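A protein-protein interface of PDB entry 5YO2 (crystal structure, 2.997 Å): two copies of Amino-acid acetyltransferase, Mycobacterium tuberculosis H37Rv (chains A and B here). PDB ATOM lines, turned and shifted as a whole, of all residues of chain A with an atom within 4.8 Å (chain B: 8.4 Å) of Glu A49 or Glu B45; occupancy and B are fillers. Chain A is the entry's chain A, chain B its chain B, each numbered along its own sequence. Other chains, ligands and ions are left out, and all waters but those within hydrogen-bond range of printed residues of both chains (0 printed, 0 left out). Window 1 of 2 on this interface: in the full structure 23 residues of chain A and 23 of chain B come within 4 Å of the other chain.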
ATOM      1  N   ARG A  14       6.058  15.541  18.443  1.00  0.00           N
ATOM      2  CA  ARG A  14       6.256  16.424  19.581  1.00  0.00           C
ATOM      3  C   ARG A  14       7.667  16.993  19.573  1.00  0.00           C
ATOM      4  O   ARG A  14       8.626  16.345  19.140  1.00  0.00           O
ATOM      5  CB  ARG A  14       6.004  15.678  20.891  1.00  0.00           C
ATOM      6  CG  ARG A  14       4.556  15.670  21.300  1.00  0.00           C
ATOM      7  CD  ARG A  14       4.310  14.861  22.556  1.00  0.00           C
ATOM      8  NE  ARG A  14       2.888  14.856  22.889  1.00  0.00           N
ATOM      9  CZ  ARG A  14       2.235  15.908  23.375  1.00  0.00           C
ATOM     10  NH1 ARG A  14       2.875  17.050  23.595  1.00  0.00           N
ATOM     11  NH2 ARG A  14       0.939  15.820  23.645  1.00  0.00           N
ATOM     12  N   ALA A  46       7.531  25.829  27.167  1.00  0.00           N
ATOM     13  CA  ALA A  46       6.377  25.403  26.391  1.00  0.00           C
ATOM     14  C   ALA A  46       6.667  24.187  25.521  1.00  0.00           C
ATOM     15  O   ALA A  46       5.813  23.801  24.717  1.00  0.00           O
ATOM     16  CB  ALA A  46       5.888  26.555  25.513  1.00  0.00           C
ATOM     17  N   VAL A  47       7.846  23.577  25.659  1.00  0.00           N
ATOM     18  CA  VAL A  47       8.229  22.491  24.766  1.00  0.00           C
ATOM     19  C   VAL A  47       7.259  21.321  24.854  1.00  0.00           C
ATOM     20  O   VAL A  47       7.141  20.546  23.900  1.00  0.00           O
ATOM     21  CB  VAL A  47       9.671  22.035  25.079  1.00  0.00           C
ATOM     22  CG1 VAL A  47       9.739  21.340  26.438  1.00  0.00           C
ATOM     23  CG2 VAL A  47      10.204  21.134  23.972  1.00  0.00           C
ATOM     24  N   GLN A  48       6.551  21.178  25.975  1.00  0.00           N
ATOM     25  CA  GLN A  48       5.666  20.037  26.170  1.00  0.00           C
ATOM     26  C   GLN A  48       4.311  20.215  25.501  1.00  0.00           C
ATOM     27  O   GLN A  48       3.513  19.270  25.497  1.00  0.00           O
ATOM     28  CB  GLN A  48       5.467  19.779  27.664  1.00  0.00           C
ATOM     29  CG  GLN A  48       6.766  19.580  28.424  1.00  0.00           C
ATOM     30  CD  GLN A  48       6.555  18.969  29.791  1.00  0.00           C
ATOM     31  OE1 GLN A  48       6.089  17.838  29.916  1.00  0.00           O
ATOM     32  NE2 GLN A  48       6.890  19.724  30.830  1.00  0.00           N
ATOM     33  N   GLU A  49       4.030  21.392  24.943  1.00  0.00           N
ATOM     34  CA  GLU A  49       2.835  21.611  24.144  1.00  0.00           C
ATOM     35  C   GLU A  49       3.162  21.958  22.701  1.00  0.00           C
ATOM     36  O   GLU A  49       2.243  22.227  21.920  1.00  0.00           O
ATOM     37  CB  GLU A  49       1.976  22.729  24.754  1.00  0.00           C
ATOM     38  CG  GLU A  49       2.645  24.093  24.765  1.00  0.00           C
ATOM     39  CD  GLU A  49       1.749  25.176  25.330  1.00  0.00           C
ATOM     40  OE1 GLU A  49       0.765  24.837  26.024  1.00  0.00           O
ATOM     41  OE2 GLU A  49       2.020  26.368  25.070  1.00  0.00           O
ATOM     42  N   PHE A  50       4.434  21.957  22.325  1.00  0.00           N
ATOM     43  CA  PHE A  50       4.835  22.337  20.982  1.00  0.00           C
ATOM     44  C   PHE A  50       4.936  21.106  20.090  1.00  0.00           C
ATOM     45  O   PHE A  50       5.142  19.982  20.552  1.00  0.00           O
ATOM     46  CB  PHE A  50       6.171  23.079  21.010  1.00  0.00           C
ATOM     47  CG  PHE A  50       6.040  24.562  20.834  1.00  0.00           C
ATOM     48  CD1 PHE A  50       5.688  25.368  21.903  1.00  0.00           C
ATOM     49  CD2 PHE A  50       6.273  25.151  19.606  1.00  0.00           C
ATOM     50  CE1 PHE A  50       5.566  26.734  21.749  1.00  0.00           C
ATOM     51  CE2 PHE A  50       6.153  26.517  19.445  1.00  0.00           C
ATOM     52  CZ  PHE A  50       5.801  27.308  20.519  1.00  0.00           C
ATOM     53  N   TRP A  51       4.794  21.343  18.788  1.00  0.00           N
ATOM     54  CA  TRP A  51       4.910  20.300  17.781  1.00  0.00           C
ATOM     55  C   TRP A  51       5.711  20.842  16.611  1.00  0.00           C
ATOM     56  O   TRP A  51       5.701  22.045  16.335  1.00  0.00           O
ATOM     57  CB  TRP A  51       3.541  19.827  17.290  1.00  0.00           C
ATOM     58  CG  TRP A  51       2.721  19.177  18.349  1.00  0.00           C
ATOM     59  CD1 TRP A  51       2.046  19.794  19.360  1.00  0.00           C
ATOM     60  CD2 TRP A  51       2.483  17.774  18.504  1.00  0.00           C
ATOM     61  NE1 TRP A  51       1.403  18.862  20.138  1.00  0.00           N
ATOM     62  CE2 TRP A  51       1.655  17.615  19.631  1.00  0.00           C
ATOM     63  CE3 TRP A  51       2.888  16.639  17.796  1.00  0.00           C
ATOM     64  CZ2 TRP A  51       1.225  16.365  20.070  1.00  0.00           C
ATOM     65  CZ3 TRP A  51       2.461  15.399  18.232  1.00  0.00           C
ATOM     66  CH2 TRP A  51       1.638  15.272  19.357  1.00  0.00           C
ATOM     67  N   GLY A  66       4.446  24.479  15.597  1.00  0.00           N
ATOM     68  CA  GLY A  66       3.091  24.830  15.965  1.00  0.00           C
ATOM     69  C   GLY A  66       2.820  24.320  17.363  1.00  0.00           C
ATOM     70  O   GLY A  66       3.481  23.395  17.848  1.00  0.00           O
ATOM     71  N   ALA A  67       1.836  24.942  18.004  1.00  0.00           N
ATOM     72  CA  ALA A  67       1.559  24.641  19.400  1.00  0.00           C
ATOM     73  C   ALA A  67       0.077  24.825  19.684  1.00  0.00           C
ATOM     74  O   ALA A  67      -0.548  25.768  19.189  1.00  0.00           O
ATOM     75  CB  ALA A  67       2.387  25.534  20.334  1.00  0.00           C
ATOM     76  N   LEU A  68      -0.479  23.907  20.468  1.00  0.00           N
ATOM     77  CA  LEU A  68      -1.829  24.049  20.993  1.00  0.00           C
ATOM     78  C   LEU A  68      -1.749  24.470  22.452  1.00  0.00           C
ATOM     79  O   LEU A  68      -1.107  23.796  23.265  1.00  0.00           O
ATOM     80  CB  LEU A  68      -2.625  22.751  20.868  1.00  0.00           C
ATOM     81  CG  LEU A  68      -4.076  22.915  21.333  1.00  0.00           C
ATOM     82  CD1 LEU A  68      -4.957  23.239  20.141  1.00  0.00           C
ATOM     83  CD2 LEU A  68      -4.582  21.686  22.062  1.00  0.00           C
ATOM     84  N   HIS A  69      -2.410  25.572  22.780  1.00  0.00           N
ATOM     85  CA  HIS A  69      -2.419  26.117  24.129  1.00  0.00           C
ATOM     86  C   HIS A  69      -3.840  26.031  24.669  1.00  0.00           C
ATOM     87  O   HIS A  69      -4.765  26.596  24.077  1.00  0.00           O
ATOM     88  CB  HIS A  69      -1.927  27.562  24.125  1.00  0.00           C
ATOM     89  CG  HIS A  69      -1.488  28.056  25.465  1.00  0.00           C
ATOM     90  ND1 HIS A  69      -0.400  27.532  26.128  1.00  0.00           N
ATOM     91  CD2 HIS A  69      -1.987  29.025  26.268  1.00  0.00           C
ATOM     92  CE1 HIS A  69      -0.247  28.156  27.282  1.00  0.00           C
ATOM     93  NE2 HIS A  69      -1.197  29.066  27.391  1.00  0.00           N
ATOM     94  N   VAL A  70      -4.014  25.326  25.787  1.00  0.00           N
ATOM     95  CA  VAL A  70      -5.322  25.260  26.422  1.00  0.00           C
ATOM     96  C   VAL A  70      -5.603  26.582  27.120  1.00  0.00           C
ATOM     97  O   VAL A  70      -4.713  27.185  27.733  1.00  0.00           O
ATOM     98  CB  VAL A  70      -5.390  24.080  27.406  1.00  0.00           C
ATOM     99  CG1 VAL A  70      -6.732  24.070  28.144  1.00  0.00           C
ATOM    100  CG2 VAL A  70      -5.171  22.769  26.677  1.00  0.00           C
ATOM    101  N   ARG A  79      -1.341  28.356  18.348  1.00  0.00           N
ATOM    102  CA  ARG A  79      -0.455  29.506  18.424  1.00  0.00           C
ATOM    103  C   ARG A  79       0.927  29.145  17.896  1.00  0.00           C
ATOM    104  O   ARG A  79       1.295  27.972  17.803  1.00  0.00           O
ATOM    105  CB  ARG A  79      -0.357  30.040  19.854  1.00  0.00           C
ATOM    106  CG  ARG A  79       0.011  29.004  20.893  1.00  0.00           C
ATOM    107  CD  ARG A  79       0.439  29.687  22.179  1.00  0.00           C
ATOM    108  NE  ARG A  79      -0.627  30.527  22.714  1.00  0.00           N
ATOM    109  CZ  ARG A  79      -0.550  31.198  23.858  1.00  0.00           C
ATOM    110  NH1 ARG A  79       0.547  31.130  24.597  1.00  0.00           N
ATOM    111  NH2 ARG A  79      -1.573  31.940  24.263  1.00  0.00           N
ATOM    112  N   SER A 146      -3.961  35.903  33.845  1.00  0.00           N
ATOM    113  CA  SER A 146      -2.868  35.162  33.234  1.00  0.00           C
ATOM    114  C   SER A 146      -1.679  36.075  32.957  1.00  0.00           C
ATOM    115  O   SER A 146      -1.833  37.269  32.688  1.00  0.00           O
ATOM    116  CB  SER A 146      -3.325  34.504  31.932  1.00  0.00           C
ATOM    117  OG  SER A 146      -2.254  33.812  31.308  1.00  0.00           O
ATOM    118  N   ASP A 148       0.250  35.284  30.422  1.00  0.00           N
ATOM    119  CA  ASP A 148       0.540  34.966  29.030  1.00  0.00           C
ATOM    120  C   ASP A 148      -0.054  36.037  28.121  1.00  0.00           C
ATOM    121  O   ASP A 148      -1.236  36.374  28.238  1.00  0.00           O
ATOM    122  CB  ASP A 148      -0.016  33.589  28.667  1.00  0.00           C
ATOM    123  CG  ASP A 148       0.353  33.162  27.257  1.00  0.00           C
ATOM    124  OD1 ASP A 148      -0.108  33.811  26.294  1.00  0.00           O
ATOM    125  OD2 ASP A 148       1.114  32.183  27.112  1.00  0.00           O
ATOM    126  N   VAL A 151      -2.991  35.052  25.755  1.00  0.00           N
ATOM    127  CA  VAL A 151      -4.306  35.060  26.386  1.00  0.00           C
ATOM    128  C   VAL A 151      -4.891  36.466  26.369  1.00  0.00           C
ATOM    129  O   VAL A 151      -6.091  36.651  26.134  1.00  0.00           O
ATOM    130  CB  VAL A 151      -4.212  34.499  27.817  1.00  0.00           C
ATOM    131  CG1 VAL A 151      -5.562  34.586  28.523  1.00  0.00           C
ATOM    132  CG2 VAL A 151      -3.712  33.066  27.790  1.00  0.00           C
ATOM    133  N   THR B  17      -8.381  18.343  31.466  1.00  0.00           N
ATOM    134  CA  THR B  17      -9.012  19.617  31.807  1.00  0.00           C
ATOM    135  C   THR B  17     -10.074  19.445  32.886  1.00  0.00           C
ATOM    136  O   THR B  17     -10.278  20.346  33.707  1.00  0.00           O
ATOM    137  CB  THR B  17      -9.631  20.270  30.566  1.00  0.00           C
ATOM    138  OG1 THR B  17     -10.508  19.344  29.909  1.00  0.00           O
ATOM    139  CG2 THR B  17      -8.547  20.737  29.601  1.00  0.00           C
ATOM    140  N   VAL B  20      -8.724  19.871  36.476  1.00  0.00           N
ATOM    141  CA  VAL B  20      -8.211  21.149  36.971  1.00  0.00           C
ATOM    142  C   VAL B  20      -8.915  21.605  38.243  1.00  0.00           C
ATOM    143  O   VAL B  20      -8.222  22.011  39.191  1.00  0.00           O
ATOM    144  CB  VAL B  20      -8.275  22.205  35.851  1.00  0.00           C
ATOM    145  CG1 VAL B  20      -8.124  23.614  36.421  1.00  0.00           C
ATOM    146  CG2 VAL B  20      -7.197  21.923  34.820  1.00  0.00           C
ATOM    147  N   ASN B  39      -3.210  30.221  39.807  1.00  0.00           N
ATOM    148  CA  ASN B  39      -4.618  30.536  39.631  1.00  0.00           C
ATOM    149  C   ASN B  39      -5.246  29.611  38.590  1.00  0.00           C
ATOM    150  O   ASN B  39      -4.572  28.823  37.923  1.00  0.00           O
ATOM    151  CB  ASN B  39      -4.800  32.005  39.247  1.00  0.00           C
ATOM    152  CG  ASN B  39      -4.030  32.390  38.000  1.00  0.00           C
ATOM    153  OD1 ASN B  39      -3.605  31.536  37.223  1.00  0.00           O
ATOM    154  ND2 ASN B  39      -3.833  33.687  37.814  1.00  0.00           N
ATOM    155  N   LEU B  40      -6.568  29.725  38.454  1.00  0.00           N
ATOM    156  CA  LEU B  40      -7.329  28.714  37.729  1.00  0.00           C
ATOM    157  C   LEU B  40      -6.944  28.670  36.254  1.00  0.00           C
ATOM    158  O   LEU B  40      -6.838  27.587  35.667  1.00  0.00           O
ATOM    159  CB  LEU B  40      -8.825  28.977  37.903  1.00  0.00           C
ATOM    160  CG  LEU B  40      -9.821  27.823  37.743  1.00  0.00           C
ATOM    161  CD1 LEU B  40      -9.264  26.478  38.187  1.00  0.00           C
ATOM    162  CD2 LEU B  40     -11.078  28.147  38.532  1.00  0.00           C
ATOM    163  N   VAL B  41      -6.747  29.833  35.631  1.00  0.00           N
ATOM    164  CA  VAL B  41      -6.434  29.858  34.204  1.00  0.00           C
ATOM    165  C   VAL B  41      -5.059  29.250  33.943  1.00  0.00           C
ATOM    166  O   VAL B  41      -4.891  28.426  33.036  1.00  0.00           O
ATOM    167  CB  VAL B  41      -6.542  31.291  33.649  1.00  0.00           C
ATOM    168  CG1 VAL B  41      -5.554  32.237  34.331  1.00  0.00           C
ATOM    169  CG2 VAL B  41      -6.336  31.289  32.137  1.00  0.00           C
ATOM    170  N   THR B  42      -4.052  29.642  34.729  1.00  0.00           N
ATOM    171  CA  THR B  42      -2.701  29.147  34.487  1.00  0.00           C
ATOM    172  C   THR B  42      -2.565  27.652  34.743  1.00  0.00           C
ATOM    173  O   THR B  42      -1.565  27.061  34.319  1.00  0.00           O
ATOM    174  CB  THR B  42      -1.683  29.909  35.344  1.00  0.00           C
ATOM    175  OG1 THR B  42      -2.060  29.844  36.723  1.00  0.00           O
ATOM    176  CG2 THR B  42      -1.591  31.368  34.897  1.00  0.00           C
ATOM    177  N   LEU B  43      -3.531  27.027  35.417  1.00  0.00           N
ATOM    178  CA  LEU B  43      -3.540  25.571  35.504  1.00  0.00           C
ATOM    179  C   LEU B  43      -4.123  24.947  34.244  1.00  0.00           C
ATOM    180  O   LEU B  43      -3.664  23.887  33.804  1.00  0.00           O
ATOM    181  CB  LEU B  43      -4.321  25.110  36.736  1.00  0.00           C
ATOM    182  CG  LEU B  43      -3.618  25.234  38.089  1.00  0.00           C
ATOM    183  CD1 LEU B  43      -4.569  24.857  39.215  1.00  0.00           C
ATOM    184  CD2 LEU B  43      -2.375  24.351  38.130  1.00  0.00           C
ATOM    185  N   TYR B  44      -5.132  25.583  33.650  1.00  0.00           N
ATOM    186  CA  TYR B  44      -5.652  25.084  32.385  1.00  0.00           C
ATOM    187  C   TYR B  44      -4.607  25.184  31.283  1.00  0.00           C
ATOM    188  O   TYR B  44      -4.575  24.342  30.381  1.00  0.00           O
ATOM    189  CB  TYR B  44      -6.920  25.847  31.993  1.00  0.00           C
ATOM    190  CG  TYR B  44      -8.156  25.369  32.721  1.00  0.00           C
ATOM    191  CD1 TYR B  44      -8.673  24.104  32.485  1.00  0.00           C
ATOM    192  CD2 TYR B  44      -8.808  26.181  33.638  1.00  0.00           C
ATOM    193  CE1 TYR B  44      -9.798  23.655  33.146  1.00  0.00           C
ATOM    194  CE2 TYR B  44      -9.939  25.742  34.305  1.00  0.00           C
ATOM    195  CZ  TYR B  44     -10.429  24.477  34.056  1.00  0.00           C
ATOM    196  OH  TYR B  44     -11.552  24.030  34.713  1.00  0.00           O
ATOM    197  N   GLU B  45      -3.730  26.189  31.351  1.00  0.00           N
ATOM    198  CA  GLU B  45      -2.671  26.321  30.357  1.00  0.00           C
ATOM    199  C   GLU B  45      -1.552  25.313  30.577  1.00  0.00           C
ATOM    200  O   GLU B  45      -0.946  24.844  29.606  1.00  0.00           O
ATOM    201  CB  GLU B  45      -2.099  27.738  30.383  1.00  0.00           C
ATOM    202  CG  GLU B  45      -3.134  28.838  30.223  1.00  0.00           C
ATOM    203  CD  GLU B  45      -2.516  30.224  30.233  1.00  0.00           C
ATOM    204  OE1 GLU B  45      -1.748  30.544  29.301  1.00  0.00           O
ATOM    205  OE2 GLU B  45      -2.786  30.991  31.182  1.00  0.00           O
ATOM    206  N   ALA B  46      -1.268  24.967  31.831  1.00  0.00           N
ATOM    207  CA  ALA B  46      -0.195  24.042  32.172  1.00  0.00           C
ATOM    208  C   ALA B  46      -0.657  22.591  32.224  1.00  0.00           C
ATOM    209  O   ALA B  46       0.123  21.719  32.622  1.00  0.00           O
ATOM    210  CB  ALA B  46       0.421  24.432  33.518  1.00  0.00           C
ATOM    211  N   VAL B  47      -1.902  22.311  31.832  1.00  0.00           N
ATOM    212  CA  VAL B  47      -2.454  20.968  31.962  1.00  0.00           C
ATOM    213  C   VAL B  47      -1.658  19.936  31.171  1.00  0.00           C
ATOM    214  O   VAL B  47      -1.708  18.743  31.492  1.00  0.00           O
ATOM    215  CB  VAL B  47      -3.936  20.975  31.529  1.00  0.00           C
ATOM    216  CG1 VAL B  47      -4.063  21.231  30.030  1.00  0.00           C
ATOM    217  CG2 VAL B  47      -4.618  19.670  31.921  1.00  0.00           C
ATOM    218  N   GLN B  48      -0.921  20.359  30.140  1.00  0.00           N
ATOM    219  CA  GLN B  48      -0.207  19.415  29.288  1.00  0.00           C
ATOM    220  C   GLN B  48       1.117  18.948  29.886  1.00  0.00           C
ATOM    221  O   GLN B  48       1.763  18.071  29.301  1.00  0.00           O
ATOM    222  CB  GLN B  48       0.034  20.034  27.906  1.00  0.00           C
ATOM    223  CG  GLN B  48      -1.250  20.507  27.221  1.00  0.00           C
ATOM    224  CD  GLN B  48      -1.084  20.750  25.728  1.00  0.00           C
ATOM    225  OE1 GLN B  48      -0.798  19.827  24.964  1.00  0.00           O
ATOM    226  NE2 GLN B  48      -1.274  21.998  25.306  1.00  0.00           N
ATOM    227  N   GLU B  49       1.535  19.504  31.028  1.00  0.00           N
ATOM    228  CA  GLU B  49       2.698  19.009  31.755  1.00  0.00           C
ATOM    229  C   GLU B  49       2.339  18.469  33.132  1.00  0.00           C
ATOM    230  O   GLU B  49       3.242  18.078  33.882  1.00  0.00           O
ATOM    231  CB  GLU B  49       3.761  20.113  31.905  1.00  0.00           C
ATOM    232  CG  GLU B  49       3.321  21.316  32.735  1.00  0.00           C
ATOM    233  CD  GLU B  49       4.425  22.350  32.908  1.00  0.00           C
ATOM    234  OE1 GLU B  49       5.404  22.321  32.131  1.00  0.00           O
ATOM    235  OE2 GLU B  49       4.312  23.194  33.824  1.00  0.00           O
ATOM    236  N   PHE B  50       1.056  18.424  33.481  1.00  0.00           N
ATOM    237  CA  PHE B  50       0.617  18.004  34.804  1.00  0.00           C
ATOM    238  C   PHE B  50       0.306  16.512  34.844  1.00  0.00           C
ATOM    239  O   PHE B  50       0.037  15.872  33.826  1.00  0.00           O
ATOM    240  CB  PHE B  50      -0.620  18.791  35.237  1.00  0.00           C
ATOM    241  CG  PHE B  50      -0.337  19.848  36.263  1.00  0.00           C
ATOM    242  CD1 PHE B  50       0.161  21.082  35.890  1.00  0.00           C
ATOM    243  CD2 PHE B  50      -0.568  19.601  37.606  1.00  0.00           C
ATOM    244  CE1 PHE B  50       0.420  22.054  36.836  1.00  0.00           C
ATOM    245  CE2 PHE B  50      -0.311  20.569  38.558  1.00  0.00           C
ATOM    246  CZ  PHE B  50       0.185  21.796  38.172  1.00  0.00           C
ATOM    247  N   VAL B  70       9.993  22.262  32.313  1.00  0.00           N
ATOM    248  CA  VAL B  70      11.279  22.410  31.652  1.00  0.00           C
ATOM    249  C   VAL B  70      11.805  23.817  31.893  1.00  0.00           C
ATOM    250  O   VAL B  70      11.048  24.798  31.875  1.00  0.00           O
ATOM    251  CB  VAL B  70      11.144  22.110  30.150  1.00  0.00           C
ATOM    252  CG1 VAL B  70      12.456  22.382  29.418  1.00  0.00           C
ATOM    253  CG2 VAL B  70      10.708  20.668  29.933  1.00  0.00           C
ATOM    254  N   LEU B 107      12.121  13.271  28.147  1.00  0.00           N
ATOM    255  CA  LEU B 107      12.509  14.564  27.601  1.00  0.00           C
ATOM    256  C   LEU B 107      14.013  14.709  27.419  1.00  0.00           C
ATOM    257  O   LEU B 107      14.469  15.785  27.017  1.00  0.00           O
ATOM    258  CB  LEU B 107      11.993  15.675  28.515  1.00  0.00           C
ATOM    259  CG  LEU B 107      10.473  15.809  28.555  1.00  0.00           C
ATOM    260  CD1 LEU B 107      10.033  16.527  29.813  1.00  0.00           C
ATOM    261  CD2 LEU B 107       9.992  16.547  27.326  1.00  0.00           C
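Among the printed residues, pairs that only touch across the chains: Val A47 with Val B70 (3.7 Å), Glu A49 with Glu B45 (3.97 Å), Glu A49 with Gln B48 (3.4 Å), Val A70 with Tyr B44 (3.1 Å), Val A70 with Glu B45 (3.4 Å), Val A70 with Val B47 (3.9 Å), Ser A146 with Val B41 (3.98 Å), Asp A148 with Glu B45 (3.6 Å) and Val A151 with Glu B45 (3.5 Å).
The backbone carbonyl oxygen (O) of Gln A48 is in hydrogen-bond range of the guanidinium group (NH1) of Arg A14 (3.0 Å). ND1 of His A69 sits at hydrogen-bond distance from OE2 of Glu A49 (2.9 Å). NH1 of Arg A79 lies within salt-bridge range of OD2 of Asp A148 (2.8 Å). OG of Ser A146 sits at hydrogen-bond distance from N of Asp A148. N of Val A151 lies within hydrogen-bond range of OD1 of Asp A148, 3.2 Å away.
Glu A49 touches just these residues of chain B: Glu B45 and Gln B48. Glu B45 touches just these residues of chain A: Glu A49, His A69, Val A70, Ser A146, Asp A148 and Val A151. Printed residues of chain B within 4 Å of Ser A146: Val B41 (3.98 Å) and Glu B45 (2.9 Å). Printed residues of chain A within 4 Å of Tyr B44: Val A70 (3.1 Å). Of the printed residues of chain A, Val B47 touches Val A70 (3.9 Å). Printed residues of chain B within 4 Å of His A69: Glu B45. Thr B42 touches none of the printed residues of chain A.
Val A47 touches Val B70, and with the chains exchanged Val A70 touches Val B47. Gln A48 touches Glu B49, and with the chains exchanged Glu A49 touches Gln B48.
Of the 16 printed residues of chain A, 9 touch a printed residue of chain B. Hydrophobic or aromatic side chains of chain A within 4 Å of the printed part of chain B: Val A47, His A69, Val A70 and Val A151. Among the printed residues, 13 pairs touch across the chains.
OE1 of Glu B49 lies within hydrogen-bond range of NE2 of Gln A48, at 3.3 Å. The side-chain amide nitrogen (NE2) of Gln B48 lies within hydrogen-bond range of the backbone carbonyl oxygen (O) of Leu A68, at 2.7 Å. NE2 of His A69 is in hydrogen-bond range of OE1 of Glu B45 (2.5 Å). OG of Ser A146 lies within hydrogen-bond range of OE2 of Glu B45.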
